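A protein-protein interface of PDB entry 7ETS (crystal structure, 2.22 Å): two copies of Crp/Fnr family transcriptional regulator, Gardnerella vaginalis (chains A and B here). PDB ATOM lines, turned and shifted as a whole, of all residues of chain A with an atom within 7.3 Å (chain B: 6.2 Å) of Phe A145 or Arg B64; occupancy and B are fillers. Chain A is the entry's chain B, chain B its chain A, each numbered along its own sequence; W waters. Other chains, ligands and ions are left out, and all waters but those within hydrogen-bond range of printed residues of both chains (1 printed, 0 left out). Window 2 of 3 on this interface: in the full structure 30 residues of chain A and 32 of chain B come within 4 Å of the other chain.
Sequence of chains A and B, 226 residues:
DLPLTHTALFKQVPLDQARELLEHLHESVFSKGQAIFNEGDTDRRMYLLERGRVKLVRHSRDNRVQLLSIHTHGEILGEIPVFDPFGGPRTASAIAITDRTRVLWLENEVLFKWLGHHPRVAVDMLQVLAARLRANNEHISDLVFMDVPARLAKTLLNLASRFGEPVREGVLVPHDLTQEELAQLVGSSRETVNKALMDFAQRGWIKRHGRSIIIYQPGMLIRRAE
Water W1 lies within hydrogen-bond range of OD1 of Asp A142, NH1 of Arg B58 and OG of Ser A141.
Among the printed residues, pairs that only touch across the chains: Phe A145 with Arg B58 (3.2 Å), Phe A145 with Arg B64 (3.4 Å), Phe A145 with Gln B66 (3.4 Å) and Phe A145 with Ser B60 (3.5 Å).
No position is printed for both chains.
OG of Ser A141 sits at hydrogen-bond distance from NH1 of Arg B58 (3.3 Å).
NH2 of Arg B61 is in hydrogen-bond range of O of Phe A145 (3.5 Å).
O of Arg B58 is in hydrogen-bond range of N of Gln B66 (3.2 Å).
The backbone carbonyl oxygen (O) of Arg B61 lies within hydrogen-bond range of the guanidinium group (NE) of Arg B64 (3.1 Å).
Printed residues of chain B that touch a printed residue of chain A: Arg B58, Ser B60, Arg B61, Arg B64 and Gln B66.
Hydrophobic or aromatic side chains of chain A that line the printed part of chain B: Phe A145.
Among the printed residues, 6 pairs touch across the chains.
Among the printed residues, no Asp or Glu carboxylate lies within 4 Å of a Lys or Arg side-chain nitrogen of the other chain.
Phe A145 touches just these residues of chain B: Arg B58 (3.2 Å), Ser B60 (3.5 Å), Arg B61 (3.5 Å), Arg B64 (3.4 Å) and Gln B66 (3.4 Å).
Of the printed residues of chain A, Arg B58 touches Ser A141 and Phe A145.
Printed residues of chain A within 4 Å of Arg B61: Phe A145.
Arg B64 touches just one residue of chain A: Phe A145 (3.4 Å).
The nearest residue of chain B that does not touch Phe A145 is His B59 (5.5 Å).
The nearest residue of chain A that does not touch Arg B64 is Val A144 (5.8 Å).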
ATOM      1  N   ILE A 140     -12.485 -15.110  -0.248  1.00  0.00           N
ATOM      2  CA  ILE A 140     -12.450 -13.667  -0.459  1.00  0.00           C
ATOM      3  C   ILE A 140     -11.495 -13.004   0.528  1.00  0.00           C
ATOM      4  O   ILE A 140     -10.859 -11.990   0.209  1.00  0.00           O
ATOM      5  CB  ILE A 140     -13.876 -13.088  -0.362  1.00  0.00           C
ATOM      6  CG1 ILE A 140     -14.762 -13.688  -1.457  1.00  0.00           C
ATOM      7  CG2 ILE A 140     -13.860 -11.570  -0.478  1.00  0.00           C
ATOM      8  CD1 ILE A 140     -16.192 -13.200  -1.419  1.00  0.00           C
ATOM      9  N   SER A 141     -11.366 -13.566   1.730  1.00  0.00           N
ATOM     10  CA  SER A 141     -10.420 -13.028   2.701  1.00  0.00           C
ATOM     11  C   SER A 141      -8.979 -13.198   2.229  1.00  0.00           C
ATOM     12  O   SER A 141      -8.113 -12.381   2.564  1.00  0.00           O
ATOM     13  CB  SER A 141     -10.622 -13.717   4.051  1.00  0.00           C
ATOM     14  OG  SER A 141     -10.140 -15.053   4.009  1.00  0.00           O
ATOM     15  N   ASP A 142      -8.706 -14.247   1.454  1.00  0.00           N
ATOM     16  CA  ASP A 142      -7.340 -14.514   1.014  1.00  0.00           C
ATOM     17  C   ASP A 142      -6.870 -13.481  -0.005  1.00  0.00           C
ATOM     18  O   ASP A 142      -5.767 -12.935   0.114  1.00  0.00           O
ATOM     19  CB  ASP A 142      -7.249 -15.925   0.431  1.00  0.00           C
ATOM     20  CG  ASP A 142      -6.831 -16.959   1.459  1.00  0.00           C
ATOM     21  OD1 ASP A 142      -6.388 -16.571   2.561  1.00  0.00           O
ATOM     22  OD2 ASP A 142      -6.942 -18.166   1.160  1.00  0.00           O
ATOM     23  N   LEU A 143      -7.702 -13.187  -1.008  1.00  0.00           N
ATOM     24  CA  LEU A 143      -7.258 -12.404  -2.156  1.00  0.00           C
ATOM     25  C   LEU A 143      -6.873 -10.970  -1.810  1.00  0.00           C
ATOM     26  O   LEU A 143      -6.292 -10.288  -2.660  1.00  0.00           O
ATOM     27  CB  LEU A 143      -8.344 -12.412  -3.233  1.00  0.00           C
ATOM     28  CG  LEU A 143      -8.344 -13.599  -4.192  1.00  0.00           C
ATOM     29  CD1 LEU A 143      -8.677 -14.904  -3.470  1.00  0.00           C
ATOM     30  CD2 LEU A 143      -9.304 -13.335  -5.337  1.00  0.00           C
ATOM     31  N   VAL A 144      -7.171 -10.494  -0.603  1.00  0.00           N
ATOM     32  CA  VAL A 144      -6.667  -9.187  -0.197  1.00  0.00           C
ATOM     33  C   VAL A 144      -5.322  -9.306   0.518  1.00  0.00           C
ATOM     34  O   VAL A 144      -4.523  -8.365   0.490  1.00  0.00           O
ATOM     35  CB  VAL A 144      -7.695  -8.446   0.678  1.00  0.00           C
ATOM     36  CG1 VAL A 144      -8.987  -8.217  -0.095  1.00  0.00           C
ATOM     37  CG2 VAL A 144      -7.961  -9.209   1.965  1.00  0.00           C
ATOM     38  N   PHE A 145      -5.048 -10.452   1.141  1.00  0.00           N
ATOM     39  CA  PHE A 145      -3.808 -10.665   1.876  1.00  0.00           C
ATOM     40  C   PHE A 145      -2.779 -11.483   1.107  1.00  0.00           C
ATOM     41  O   PHE A 145      -1.595 -11.442   1.457  1.00  0.00           O
ATOM     42  CB  PHE A 145      -4.098 -11.364   3.210  1.00  0.00           C
ATOM     43  CG  PHE A 145      -4.597 -10.441   4.283  1.00  0.00           C
ATOM     44  CD1 PHE A 145      -4.049  -9.179   4.441  1.00  0.00           C
ATOM     45  CD2 PHE A 145      -5.617 -10.832   5.134  1.00  0.00           C
ATOM     46  CE1 PHE A 145      -4.505  -8.327   5.428  1.00  0.00           C
ATOM     47  CE2 PHE A 145      -6.078  -9.983   6.121  1.00  0.00           C
ATOM     48  CZ  PHE A 145      -5.520  -8.732   6.269  1.00  0.00           C
ATOM     49  N   MET A 146      -3.195 -12.217   0.078  1.00  0.00           N
ATOM     50  CA  MET A 146      -2.299 -13.104  -0.651  1.00  0.00           C
ATOM     51  C   MET A 146      -1.646 -12.368  -1.812  1.00  0.00           C
ATOM     52  O   MET A 146      -2.321 -11.667  -2.574  1.00  0.00           O
ATOM     53  CB  MET A 146      -3.051 -14.336  -1.164  1.00  0.00           C
ATOM     54  CG  MET A 146      -3.580 -15.244  -0.064  1.00  0.00           C
ATOM     55  SD  MET A 146      -3.759 -16.964  -0.582  1.00  0.00           S
ATOM     56  CE  MET A 146      -4.832 -16.793  -2.005  1.00  0.00           C
ATOM     57  N   ASP A 147      -0.332 -12.526  -1.938  1.00  0.00           N
ATOM     58  CA  ASP A 147       0.384 -12.030  -3.101  1.00  0.00           C
ATOM     59  C   ASP A 147       0.251 -13.031  -4.246  1.00  0.00           C
ATOM     60  O   ASP A 147      -0.438 -14.052  -4.135  1.00  0.00           O
ATOM     61  CB  ASP A 147       1.844 -11.753  -2.747  1.00  0.00           C
ATOM     62  CG  ASP A 147       2.560 -12.978  -2.211  1.00  0.00           C
ATOM     63  OD1 ASP A 147       1.879 -13.951  -1.827  1.00  0.00           O
ATOM     64  OD2 ASP A 147       3.807 -12.966  -2.169  1.00  0.00           O
ATOM     65  N   ALA A 150       1.213 -16.763  -3.554  1.00  0.00           N
ATOM     66  CA  ALA A 150       0.264 -17.437  -2.672  1.00  0.00           C
ATOM     67  C   ALA A 150      -0.975 -17.885  -3.436  1.00  0.00           C
ATOM     68  O   ALA A 150      -1.452 -19.010  -3.251  1.00  0.00           O
ATOM     69  CB  ALA A 150      -0.119 -16.519  -1.512  1.00  0.00           C
ATOM     70  N   ARG A 151      -1.511 -17.021  -4.303  1.00  0.00           N
ATOM     71  CA  ARG A 151      -2.681 -17.407  -5.084  1.00  0.00           C
ATOM     72  C   ARG A 151      -2.337 -18.471  -6.117  1.00  0.00           C
ATOM     73  O   ARG A 151      -3.173 -19.329  -6.422  1.00  0.00           O
ATOM     74  CB  ARG A 151      -3.288 -16.186  -5.770  1.00  0.00           C
ATOM     75  CG  ARG A 151      -3.630 -15.036  -4.832  1.00  0.00           C
ATOM     76  CD  ARG A 151      -4.541 -14.058  -5.529  1.00  0.00           C
ATOM     77  NE  ARG A 151      -3.972 -13.617  -6.792  1.00  0.00           N
ATOM     78  CZ  ARG A 151      -3.780 -12.346  -7.131  1.00  0.00           C
ATOM     79  NH1 ARG A 151      -4.134 -11.382  -6.303  1.00  0.00           N
ATOM     80  NH2 ARG A 151      -3.265 -12.033  -8.317  1.00  0.00           N
ATOM     81  N   GLU A 226      -0.144 -19.733   2.822  1.00  0.00           N
ATOM     82  CA  GLU A 226      -0.569 -19.040   4.037  1.00  0.00           C
ATOM     83  C   GLU A 226      -0.179 -17.567   3.989  1.00  0.00           C
ATOM     84  O   GLU A 226      -1.038 -16.685   4.016  1.00  0.00           O
ATOM     85  CB  GLU A 226       0.030 -19.703   5.280  1.00  0.00           C
ATOM     86  CG  GLU A 226      -0.622 -21.023   5.659  1.00  0.00           C
ATOM     87  CD  GLU A 226      -2.069 -20.855   6.091  1.00  0.00           C
ATOM     88  OE1 GLU A 226      -2.422 -19.766   6.593  1.00  0.00           O
ATOM     89  OE2 GLU A 226      -2.855 -21.810   5.925  1.00  0.00           O
ATOM     90  N   ARG B  58     -10.519  -8.297  10.581  1.00  0.00           N
ATOM     91  CA  ARG B  58      -9.633  -9.403  10.228  1.00  0.00           C
ATOM     92  C   ARG B  58      -8.185  -8.975  10.527  1.00  0.00           C
ATOM     93  O   ARG B  58      -7.532  -8.353   9.695  1.00  0.00           O
ATOM     94  CB  ARG B  58      -9.830  -9.778   8.770  1.00  0.00           C
ATOM     95  CG  ARG B  58      -8.917 -10.849   8.237  1.00  0.00           C
ATOM     96  CD  ARG B  58      -9.288 -11.187   6.796  1.00  0.00           C
ATOM     97  NE  ARG B  58      -8.387 -12.182   6.230  1.00  0.00           N
ATOM     98  CZ  ARG B  58      -8.453 -13.482   6.495  1.00  0.00           C
ATOM     99  NH1 ARG B  58      -7.597 -14.324   5.929  1.00  0.00           N
ATOM    100  NH2 ARG B  58      -9.381 -13.943   7.322  1.00  0.00           N
ATOM    101  N   HIS B  59      -7.721  -9.323  11.725  1.00  0.00           N
ATOM    102  CA  HIS B  59      -6.338  -9.090  12.127  1.00  0.00           C
ATOM    103  C   HIS B  59      -5.477 -10.239  11.616  1.00  0.00           C
ATOM    104  O   HIS B  59      -5.674 -11.393  12.014  1.00  0.00           O
ATOM    105  CB  HIS B  59      -6.229  -8.969  13.647  1.00  0.00           C
ATOM    106  CG  HIS B  59      -7.195  -7.996  14.250  1.00  0.00           C
ATOM    107  ND1 HIS B  59      -6.812  -6.754  14.707  1.00  0.00           N
ATOM    108  CD2 HIS B  59      -8.525  -8.089  14.489  1.00  0.00           C
ATOM    109  CE1 HIS B  59      -7.863  -6.120  15.193  1.00  0.00           C
ATOM    110  NE2 HIS B  59      -8.916  -6.907  15.072  1.00  0.00           N
ATOM    111  N   SER B  60      -4.529  -9.928  10.732  1.00  0.00           N
ATOM    112  CA  SER B  60      -3.712 -10.969  10.122  1.00  0.00           C
ATOM    113  C   SER B  60      -2.251 -10.559  10.032  1.00  0.00           C
ATOM    114  O   SER B  60      -1.505 -10.647  11.015  1.00  0.00           O
ATOM    115  CB  SER B  60      -4.245 -11.306   8.728  1.00  0.00           C
ATOM    116  OG  SER B  60      -3.477 -12.317   8.096  1.00  0.00           O
ATOM    117  N   ARG B  61      -1.835 -10.125   8.848  1.00  0.00           N
ATOM    118  CA  ARG B  61      -0.432  -9.823   8.611  1.00  0.00           C
ATOM    119  C   ARG B  61      -0.006  -8.645   9.463  1.00  0.00           C
ATOM    120  O   ARG B  61      -0.586  -7.557   9.363  1.00  0.00           O
ATOM    121  CB  ARG B  61      -0.195  -9.494   7.141  1.00  0.00           C
ATOM    122  CG  ARG B  61       1.259  -9.281   6.770  1.00  0.00           C
ATOM    123  CD  ARG B  61       1.384  -8.915   5.317  1.00  0.00           C
ATOM    124  NE  ARG B  61       0.952 -10.027   4.478  1.00  0.00           N
ATOM    125  CZ  ARG B  61       1.725 -11.048   4.129  1.00  0.00           C
ATOM    126  NH1 ARG B  61       2.979 -11.117   4.553  1.00  0.00           N
ATOM    127  NH2 ARG B  61       1.235 -12.009   3.360  1.00  0.00           N
ATOM    128  N   ASP B  62       1.012  -8.864  10.299  1.00  0.00           N
ATOM    129  CA  ASP B  62       1.588  -7.810  11.126  1.00  0.00           C
ATOM    130  C   ASP B  62       0.565  -7.268  12.121  1.00  0.00           C
ATOM    131  O   ASP B  62       0.778  -6.211  12.742  1.00  0.00           O
ATOM    132  CB  ASP B  62       2.156  -6.669  10.263  1.00  0.00           C
ATOM    133  CG  ASP B  62       3.626  -6.847   9.943  1.00  0.00           C
ATOM    134  OD1 ASP B  62       4.096  -7.994  10.091  1.00  0.00           O
ATOM    135  OD2 ASP B  62       4.306  -5.877   9.557  1.00  0.00           O
ATOM    136  N   ASN B  63      -0.551  -7.992  12.257  1.00  0.00           N
ATOM    137  CA  ASN B  63      -1.698  -7.576  13.059  1.00  0.00           C
ATOM    138  C   ASN B  63      -2.246  -6.248  12.533  1.00  0.00           C
ATOM    139  O   ASN B  63      -2.408  -5.272  13.271  1.00  0.00           O
ATOM    140  CB  ASN B  63      -1.325  -7.499  14.545  1.00  0.00           C
ATOM    141  CG  ASN B  63      -1.103  -8.871  15.191  1.00  0.00           C
ATOM    142  OD1 ASN B  63      -1.612  -9.881  14.703  1.00  0.00           O
ATOM    143  ND2 ASN B  63      -0.309  -8.916  16.256  1.00  0.00           N
ATOM    144  N   ARG B  64      -2.484  -6.212  11.221  1.00  0.00           N
ATOM    145  CA  ARG B  64      -3.115  -5.078  10.559  1.00  0.00           C
ATOM    146  C   ARG B  64      -4.604  -5.365  10.448  1.00  0.00           C
ATOM    147  O   ARG B  64      -5.001  -6.416   9.938  1.00  0.00           O
ATOM    148  CB  ARG B  64      -2.506  -4.837   9.177  1.00  0.00           C
ATOM    149  CG  ARG B  64      -1.045  -4.413   9.183  1.00  0.00           C
ATOM    150  CD  ARG B  64      -0.484  -4.324   7.765  1.00  0.00           C
ATOM    151  NE  ARG B  64      -0.705  -5.556   7.009  1.00  0.00           N
ATOM    152  CZ  ARG B  64      -1.359  -5.625   5.853  1.00  0.00           C
ATOM    153  NH1 ARG B  64      -1.853  -4.528   5.294  1.00  0.00           N
ATOM    154  NH2 ARG B  64      -1.509  -6.795   5.246  1.00  0.00           N
ATOM    155  N   VAL B  65      -5.424  -4.450  10.956  1.00  0.00           N
ATOM    156  CA  VAL B  65      -6.862  -4.653  10.900  1.00  0.00           C
ATOM    157  C   VAL B  65      -7.329  -4.428   9.468  1.00  0.00           C
ATOM    158  O   VAL B  65      -6.905  -3.479   8.795  1.00  0.00           O
ATOM    159  CB  VAL B  65      -7.586  -3.740  11.905  1.00  0.00           C
ATOM    160  CG1 VAL B  65      -7.475  -2.270  11.513  1.00  0.00           C
ATOM    161  CG2 VAL B  65      -9.038  -4.165  12.056  1.00  0.00           C
ATOM    162  N   GLN B  66      -8.165  -5.337   8.975  1.00  0.00           N
ATOM    163  CA  GLN B  66      -8.634  -5.309   7.593  1.00  0.00           C
ATOM    164  C   GLN B  66     -10.153  -5.390   7.604  1.00  0.00           C
ATOM    165  O   GLN B  66     -10.721  -6.416   7.989  1.00  0.00           O
ATOM    166  CB  GLN B  66      -8.021  -6.454   6.783  1.00  0.00           C
ATOM    167  CG  GLN B  66      -8.584  -6.627   5.381  1.00  0.00           C
ATOM    168  CD  GLN B  66      -8.198  -5.503   4.437  1.00  0.00           C
ATOM    169  OE1 GLN B  66      -7.156  -4.870   4.602  1.00  0.00           O
ATOM    170  NE2 GLN B  66      -9.039  -5.255   3.436  1.00  0.00           N
ATOM    171  N   LEU B  68     -13.737  -6.038   6.457  1.00  0.00           N
ATOM    172  CA  LEU B  68     -14.378  -6.933   5.502  1.00  0.00           C
ATOM    173  C   LEU B  68     -15.807  -6.527   5.179  1.00  0.00           C
ATOM    174  O   LEU B  68     -16.231  -6.635   4.025  1.00  0.00           O
ATOM    175  CB  LEU B  68     -14.374  -8.370   6.035  1.00  0.00           C
ATOM    176  CG  LEU B  68     -13.056  -8.936   6.572  1.00  0.00           C
ATOM    177  CD1 LEU B  68     -13.230 -10.402   6.952  1.00  0.00           C
ATOM    178  CD2 LEU B  68     -11.939  -8.760   5.557  1.00  0.00           C
HETATM  179  O   HOH W   1      -7.781 -16.553   4.683  1.00  0.00           O
